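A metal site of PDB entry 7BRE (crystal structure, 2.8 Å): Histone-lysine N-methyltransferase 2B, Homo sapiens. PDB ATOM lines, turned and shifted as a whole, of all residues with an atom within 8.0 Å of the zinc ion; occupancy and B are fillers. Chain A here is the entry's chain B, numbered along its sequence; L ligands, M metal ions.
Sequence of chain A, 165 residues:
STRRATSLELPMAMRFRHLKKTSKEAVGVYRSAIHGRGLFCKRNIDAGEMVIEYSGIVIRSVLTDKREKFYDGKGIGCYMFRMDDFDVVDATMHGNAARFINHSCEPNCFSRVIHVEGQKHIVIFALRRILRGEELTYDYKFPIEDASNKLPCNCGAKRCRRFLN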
ATOM      1  N   ILE A  34     -36.401   9.672 -15.916  1.00  0.00           N
ATOM      2  CA  ILE A  34     -35.099  10.260 -15.605  1.00  0.00           C
ATOM      3  C   ILE A  34     -35.175  11.762 -15.857  1.00  0.00           C
ATOM      4  O   ILE A  34     -34.962  12.564 -14.944  1.00  0.00           O
ATOM      5  CB  ILE A  34     -33.977   9.624 -16.447  1.00  0.00           C
ATOM      6  CG1 ILE A  34     -33.712   8.182 -16.012  1.00  0.00           C
ATOM      7  CG2 ILE A  34     -32.717  10.443 -16.373  1.00  0.00           C
ATOM      8  CD1 ILE A  34     -32.821   7.407 -16.956  1.00  0.00           C
ATOM      9  N   HIS A 103     -28.584   9.839 -19.897  1.00  0.00           N
ATOM     10  CA  HIS A 103     -27.407   9.253 -19.272  1.00  0.00           C
ATOM     11  C   HIS A 103     -27.807   8.390 -18.090  1.00  0.00           C
ATOM     12  O   HIS A 103     -28.807   8.654 -17.409  1.00  0.00           O
ATOM     13  CB  HIS A 103     -26.430  10.338 -18.799  1.00  0.00           C
ATOM     14  CG  HIS A 103     -25.404   9.853 -17.834  1.00  0.00           C
ATOM     15  ND1 HIS A 103     -24.134   9.471 -18.219  1.00  0.00           N
ATOM     16  CD2 HIS A 103     -25.462   9.669 -16.487  1.00  0.00           C
ATOM     17  CE1 HIS A 103     -23.453   9.090 -17.149  1.00  0.00           C
ATOM     18  NE2 HIS A 103     -24.236   9.196 -16.091  1.00  0.00           N
ATOM     19  N   SER A 104     -27.023   7.343 -17.854  1.00  0.00           N
ATOM     20  CA  SER A 104     -27.054   6.620 -16.583  1.00  0.00           C
ATOM     21  C   SER A 104     -25.639   6.309 -16.166  1.00  0.00           C
ATOM     22  O   SER A 104     -24.703   6.286 -16.978  1.00  0.00           O
ATOM     23  CB  SER A 104     -27.871   5.329 -16.656  1.00  0.00           C
ATOM     24  OG  SER A 104     -28.137   4.805 -15.378  1.00  0.00           O
ATOM     25  N   CYS A 105     -25.486   6.084 -14.859  1.00  0.00           N
ATOM     26  CA  CYS A 105     -24.296   5.439 -14.330  1.00  0.00           C
ATOM     27  C   CYS A 105     -24.380   3.921 -14.465  1.00  0.00           C
ATOM     28  O   CYS A 105     -23.350   3.245 -14.336  1.00  0.00           O
ATOM     29  CB  CYS A 105     -24.105   5.833 -12.871  1.00  0.00           C
ATOM     30  SG  CYS A 105     -24.484   7.569 -12.535  1.00  0.00           S
ATOM     31  N   GLU A 106     -25.571   3.393 -14.751  1.00  0.00           N
ATOM     32  CA  GLU A 106     -25.805   1.960 -14.917  1.00  0.00           C
ATOM     33  C   GLU A 106     -26.414   1.700 -16.289  1.00  0.00           C
ATOM     34  O   GLU A 106     -27.495   1.116 -16.402  1.00  0.00           O
ATOM     35  CB  GLU A 106     -26.736   1.444 -13.824  1.00  0.00           C
ATOM     36  CG  GLU A 106     -26.516  -0.005 -13.425  1.00  0.00           C
ATOM     37  CD  GLU A 106     -26.853  -0.246 -11.963  1.00  0.00           C
ATOM     38  OE1 GLU A 106     -26.008   0.034 -11.097  1.00  0.00           O
ATOM     39  OE2 GLU A 106     -27.991  -0.702 -11.693  1.00  0.00           O
ATOM     40  N   LEU A 151     -23.746  18.977 -12.321  1.00  0.00           N
ATOM     41  CA  LEU A 151     -25.034  18.640 -12.918  1.00  0.00           C
ATOM     42  C   LEU A 151     -25.602  17.426 -12.223  1.00  0.00           C
ATOM     43  O   LEU A 151     -25.036  16.334 -12.330  1.00  0.00           O
ATOM     44  CB  LEU A 151     -24.888  18.387 -14.419  1.00  0.00           C
ATOM     45  CG  LEU A 151     -26.063  18.687 -15.353  1.00  0.00           C
ATOM     46  CD1 LEU A 151     -25.603  18.608 -16.800  1.00  0.00           C
ATOM     47  CD2 LEU A 151     -27.246  17.757 -15.113  1.00  0.00           C
ATOM     48  N   PRO A 152     -26.728  17.542 -11.508  1.00  0.00           N
ATOM     49  CA  PRO A 152     -27.271  16.386 -10.801  1.00  0.00           C
ATOM     50  C   PRO A 152     -27.838  15.356 -11.769  1.00  0.00           C
ATOM     51  O   PRO A 152     -28.513  15.695 -12.738  1.00  0.00           O
ATOM     52  CB  PRO A 152     -28.383  16.988  -9.924  1.00  0.00           C
ATOM     53  CG  PRO A 152     -28.799  18.223 -10.664  1.00  0.00           C
ATOM     54  CD  PRO A 152     -27.551  18.748 -11.319  1.00  0.00           C
ATOM     55  N   CYS A 153     -27.551  14.084 -11.494  1.00  0.00           N
ATOM     56  CA  CYS A 153     -28.066  12.971 -12.277  1.00  0.00           C
ATOM     57  C   CYS A 153     -29.291  12.364 -11.608  1.00  0.00           C
ATOM     58  O   CYS A 153     -29.388  12.309 -10.378  1.00  0.00           O
ATOM     59  CB  CYS A 153     -27.000  11.897 -12.469  1.00  0.00           C
ATOM     60  SG  CYS A 153     -27.616  10.426 -13.329  1.00  0.00           S
ATOM     61  N   ASN A 154     -30.212  11.884 -12.442  1.00  0.00           N
ATOM     62  CA  ASN A 154     -31.484  11.308 -11.992  1.00  0.00           C
ATOM     63  C   ASN A 154     -31.700   9.908 -12.564  1.00  0.00           C
ATOM     64  O   ASN A 154     -32.842   9.469 -12.683  1.00  0.00           O
ATOM     65  CB  ASN A 154     -32.651  12.228 -12.359  1.00  0.00           C
ATOM     66  CG  ASN A 154     -33.894  11.983 -11.518  1.00  0.00           C
ATOM     67  OD1 ASN A 154     -33.798  11.618 -10.340  1.00  0.00           O
ATOM     68  ND2 ASN A 154     -35.063  12.180 -12.116  1.00  0.00           N
ATOM     69  N   CYS A 155     -30.612   9.211 -12.913  1.00  0.00           N
ATOM     70  CA  CYS A 155     -30.736   7.896 -13.542  1.00  0.00           C
ATOM     71  C   CYS A 155     -31.423   6.881 -12.637  1.00  0.00           C
ATOM     72  O   CYS A 155     -31.873   5.840 -13.121  1.00  0.00           O
ATOM     73  CB  CYS A 155     -29.358   7.377 -13.958  1.00  0.00           C
ATOM     74  SG  CYS A 155     -28.163   7.195 -12.615  1.00  0.00           S
ATOM     75  N   GLY A 156     -31.513   7.161 -11.336  1.00  0.00           N
ATOM     76  CA  GLY A 156     -32.356   6.404 -10.438  1.00  0.00           C
ATOM     77  C   GLY A 156     -31.932   4.977 -10.161  1.00  0.00           C
ATOM     78  O   GLY A 156     -32.703   4.231  -9.560  1.00  0.00           O
ATOM     79  N   ALA A 157     -30.739   4.584 -10.592  1.00  0.00           N
ATOM     80  CA  ALA A 157     -30.191   3.274 -10.275  1.00  0.00           C
ATOM     81  C   ALA A 157     -29.175   3.401  -9.150  1.00  0.00           C
ATOM     82  O   ALA A 157     -28.482   4.411  -9.048  1.00  0.00           O
ATOM     83  CB  ALA A 157     -29.548   2.632 -11.501  1.00  0.00           C
ATOM     84  N   LYS A 158     -29.088   2.377  -8.314  1.00  0.00           N
ATOM     85  CA  LYS A 158     -28.111   2.400  -7.240  1.00  0.00           C
ATOM     86  C   LYS A 158     -26.702   2.315  -7.814  1.00  0.00           C
ATOM     87  O   LYS A 158     -26.482   1.891  -8.953  1.00  0.00           O
ATOM     88  CB  LYS A 158     -28.360   1.274  -6.231  1.00  0.00           C
ATOM     89  CG  LYS A 158     -28.227  -0.132  -6.794  1.00  0.00           C
ATOM     90  CD  LYS A 158     -29.321  -1.028  -6.230  1.00  0.00           C
ATOM     91  CE  LYS A 158     -30.539  -1.034  -7.137  1.00  0.00           C
ATOM     92  NZ  LYS A 158     -30.183  -1.635  -8.451  1.00  0.00           N
ATOM     93  N   ARG A 159     -25.730   2.728  -6.997  1.00  0.00           N
ATOM     94  CA  ARG A 159     -24.349   3.016  -7.394  1.00  0.00           C
ATOM     95  C   ARG A 159     -24.253   4.231  -8.324  1.00  0.00           C
ATOM     96  O   ARG A 159     -23.226   4.418  -8.978  1.00  0.00           O
ATOM     97  CB  ARG A 159     -23.657   1.818  -8.064  1.00  0.00           C
ATOM     98  CG  ARG A 159     -24.027   0.417  -7.577  1.00  0.00           C
ATOM     99  CD  ARG A 159     -23.676   0.169  -6.130  1.00  0.00           C
ATOM    100  NE  ARG A 159     -23.851  -1.243  -5.802  1.00  0.00           N
ATOM    101  CZ  ARG A 159     -24.030  -1.717  -4.572  1.00  0.00           C
ATOM    102  NH1 ARG A 159     -24.048  -0.885  -3.535  1.00  0.00           N
ATOM    103  NH2 ARG A 159     -24.190  -3.017  -4.373  1.00  0.00           N
ATOM    104  N   CYS A 160     -25.303   5.044  -8.393  1.00  0.00           N
ATOM    105  CA  CYS A 160     -25.281   6.234  -9.226  1.00  0.00           C
ATOM    106  C   CYS A 160     -24.298   7.263  -8.696  1.00  0.00           C
ATOM    107  O   CYS A 160     -24.268   7.562  -7.499  1.00  0.00           O
ATOM    108  CB  CYS A 160     -26.680   6.853  -9.300  1.00  0.00           C
ATOM    109  SG  CYS A 160     -26.729   8.567  -9.883  1.00  0.00           S
ATOM    110  N   ARG A 161     -23.500   7.842  -9.598  1.00  0.00           N
ATOM    111  CA  ARG A 161     -22.427   8.761  -9.240  1.00  0.00           C
ATOM    112  C   ARG A 161     -22.913  10.107  -8.706  1.00  0.00           C
ATOM    113  O   ARG A 161     -22.072  10.967  -8.405  1.00  0.00           O
ATOM    114  CB  ARG A 161     -21.518   8.984 -10.449  1.00  0.00           C
ATOM    115  CG  ARG A 161     -20.626   7.791 -10.765  1.00  0.00           C
ATOM    116  CD  ARG A 161     -20.618   7.446 -12.244  1.00  0.00           C
ATOM    117  NE  ARG A 161     -20.458   6.011 -12.462  1.00  0.00           N
ATOM    118  CZ  ARG A 161     -20.718   5.396 -13.610  1.00  0.00           C
ATOM    119  NH1 ARG A 161     -20.555   4.089 -13.715  1.00  0.00           N
ATOM    120  NH2 ARG A 161     -21.123   6.098 -14.662  1.00  0.00           N
ATOM    121  N   ARG A 162     -24.226  10.314  -8.615  1.00  0.00           N
ATOM    122  CA  ARG A 162     -24.922  11.450  -8.024  1.00  0.00           C
ATOM    123  C   ARG A 162     -24.844  12.698  -8.902  1.00  0.00           C
ATOM    124  O   ARG A 162     -25.544  13.669  -8.615  1.00  0.00           O
ATOM    125  CB  ARG A 162     -24.422  11.801  -6.604  1.00  0.00           C
ATOM    126  CG  ARG A 162     -25.410  12.527  -5.710  1.00  0.00           C
ATOM    127  CD  ARG A 162     -24.711  13.721  -5.066  1.00  0.00           C
ATOM    128  NE  ARG A 162     -25.332  14.147  -3.819  1.00  0.00           N
ATOM    129  CZ  ARG A 162     -26.424  14.909  -3.750  1.00  0.00           C
ATOM    130  NH1 ARG A 162     -27.016  15.316  -4.860  1.00  0.00           N
ATOM    131  NH2 ARG A 162     -26.910  15.266  -2.575  1.00  0.00           N
ATOM    132  N   PHE A 163     -24.073  12.700  -9.986  1.00  0.00           N
ATOM    133  CA  PHE A 163     -23.921  13.872 -10.828  1.00  0.00           C
ATOM    134  C   PHE A 163     -23.530  13.457 -12.232  1.00  0.00           C
ATOM    135  O   PHE A 163     -22.784  12.490 -12.422  1.00  0.00           O
ATOM    136  CB  PHE A 163     -22.856  14.837 -10.275  1.00  0.00           C
ATOM    137  CG  PHE A 163     -23.277  15.556  -9.011  1.00  0.00           C
ATOM    138  CD1 PHE A 163     -24.380  16.390  -9.002  1.00  0.00           C
ATOM    139  CD2 PHE A 163     -22.537  15.420  -7.847  1.00  0.00           C
ATOM    140  CE1 PHE A 163     -24.752  17.053  -7.838  1.00  0.00           C
ATOM    141  CE2 PHE A 163     -22.895  16.086  -6.687  1.00  0.00           C
ATOM    142  CZ  PHE A 163     -24.012  16.903  -6.689  1.00  0.00           C
ATOM    143  N   LEU A 164     -24.029  14.201 -13.228  1.00  0.00           N
ATOM    144  CA  LEU A 164     -23.646  13.951 -14.615  1.00  0.00           C
ATOM    145  C   LEU A 164     -22.174  14.264 -14.865  1.00  0.00           C
ATOM    146  O   LEU A 164     -21.616  13.780 -15.853  1.00  0.00           O
ATOM    147  CB  LEU A 164     -24.504  14.791 -15.569  1.00  0.00           C
ATOM    148  CG  LEU A 164     -25.929  14.291 -15.858  1.00  0.00           C
ATOM    149  CD1 LEU A 164     -26.400  14.759 -17.230  1.00  0.00           C
ATOM    150  CD2 LEU A 164     -25.984  12.785 -15.776  1.00  0.00           C
HETATM  151  N1  LIG L   1     -34.019  14.145 -21.697  1.00  0.00           N
HETATM  152  C1  LIG L   1     -33.370  14.968 -22.706  1.00  0.00           C
HETATM  153  C2  LIG L   1     -32.590  14.095 -23.681  1.00  0.00           C
HETATM  154  C3  LIG L   1     -31.081  14.142 -23.486  1.00  0.00           C
HETATM  155  S1  LIG L   1     -30.375  15.694 -24.068  1.00  0.00           S
HETATM  156  C4  LIG L   1     -34.392  15.828 -23.455  1.00  0.00           C
HETATM  157  O1  LIG L   1     -34.032  16.625 -24.325  1.00  0.00           O
HETATM  158  O2  LIG L   1     -35.591  15.734 -23.211  1.00  0.00           O
HETATM  159  C5  LIG L   1     -29.256  15.740 -22.644  1.00  0.00           C
HETATM  160  C6  LIG L   1     -29.779  16.615 -21.512  1.00  0.00           C
HETATM  161  O3  LIG L   1     -30.700  15.879 -20.723  1.00  0.00           O
HETATM  162  C7  LIG L   1     -28.665  17.091 -20.600  1.00  0.00           C
HETATM  163  O4  LIG L   1     -28.425  18.462 -20.801  1.00  0.00           O
HETATM  164  C8  LIG L   1     -29.160  16.856 -19.190  1.00  0.00           C
HETATM  165  O5  LIG L   1     -29.499  18.080 -18.586  1.00  0.00           O
HETATM  166  C9  LIG L   1     -30.416  16.024 -19.352  1.00  0.00           C
HETATM  167  N2  LIG L   1     -30.146  14.701 -18.751  1.00  0.00           N
HETATM  168  C10 LIG L   1     -29.685  13.596 -19.405  1.00  0.00           C
HETATM  169  N3  LIG L   1     -29.557  12.594 -18.505  1.00  0.00           N
HETATM  170  C11 LIG L   1     -29.924  13.054 -17.290  1.00  0.00           C
HETATM  171  C12 LIG L   1     -29.984  12.459 -16.037  1.00  0.00           C
HETATM  172  N4  LIG L   1     -29.627  11.186 -15.903  1.00  0.00           N
HETATM  173  N5  LIG L   1     -30.403  13.193 -14.959  1.00  0.00           N
HETATM  174  C13 LIG L   1     -30.761  14.519 -15.105  1.00  0.00           C
HETATM  175  N6  LIG L   1     -30.705  15.107 -16.351  1.00  0.00           N
HETATM  176  C14 LIG L   1     -30.296  14.384 -17.425  1.00  0.00           C
HETATM  177 ZN    ZN M   1     -26.508   8.777 -12.259  1.00  0.00          ZN
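The zinc ion is bound by SG of Cys 153 (2.3 Å).
SG of Cys 155 binds the zinc ion (2.3 Å).
SG of Cys 105 binds the zinc ion.
SG of Cys 160 binds the zinc ion (2.4 Å).
The zinc ion has four donor atoms within binding distance.
The backbone NH (N) of Asn 154 sits at hydrogen-bond distance from a nitrogen (N5) of the ligand (2.8 Å).
The side-chain sulfur (SG) of Cys 153 sits close to a nitrogen (N4) of the ligand.
The backbone NH (N) of His 103 lies within hydrogen-bond range of a nitrogen (N3) of the ligand (3.2 Å).
The backbone carbonyl oxygen of His 103 is in hydrogen-bond range of a nitrogen (N4) of the ligand, 3.1 Å away.
Of the 19 residues printed, 4 come within 4 Å of the zinc ion.
The nearest printed residue that does not touch the zinc ion is Arg 161 (4.1 Å).
The backbone carbonyl oxygen (O) of Cys 105 is in hydrogen-bond range of the guanidinium group (NH1) of Arg 161 (3.0 Å).
The side-chain hydroxyl of Ser 104 sits close to the side-chain sulfur of Cys 155 (3.7 Å).
SG of Cys 160 sits close to N of Arg 162, at 3.3 Å.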
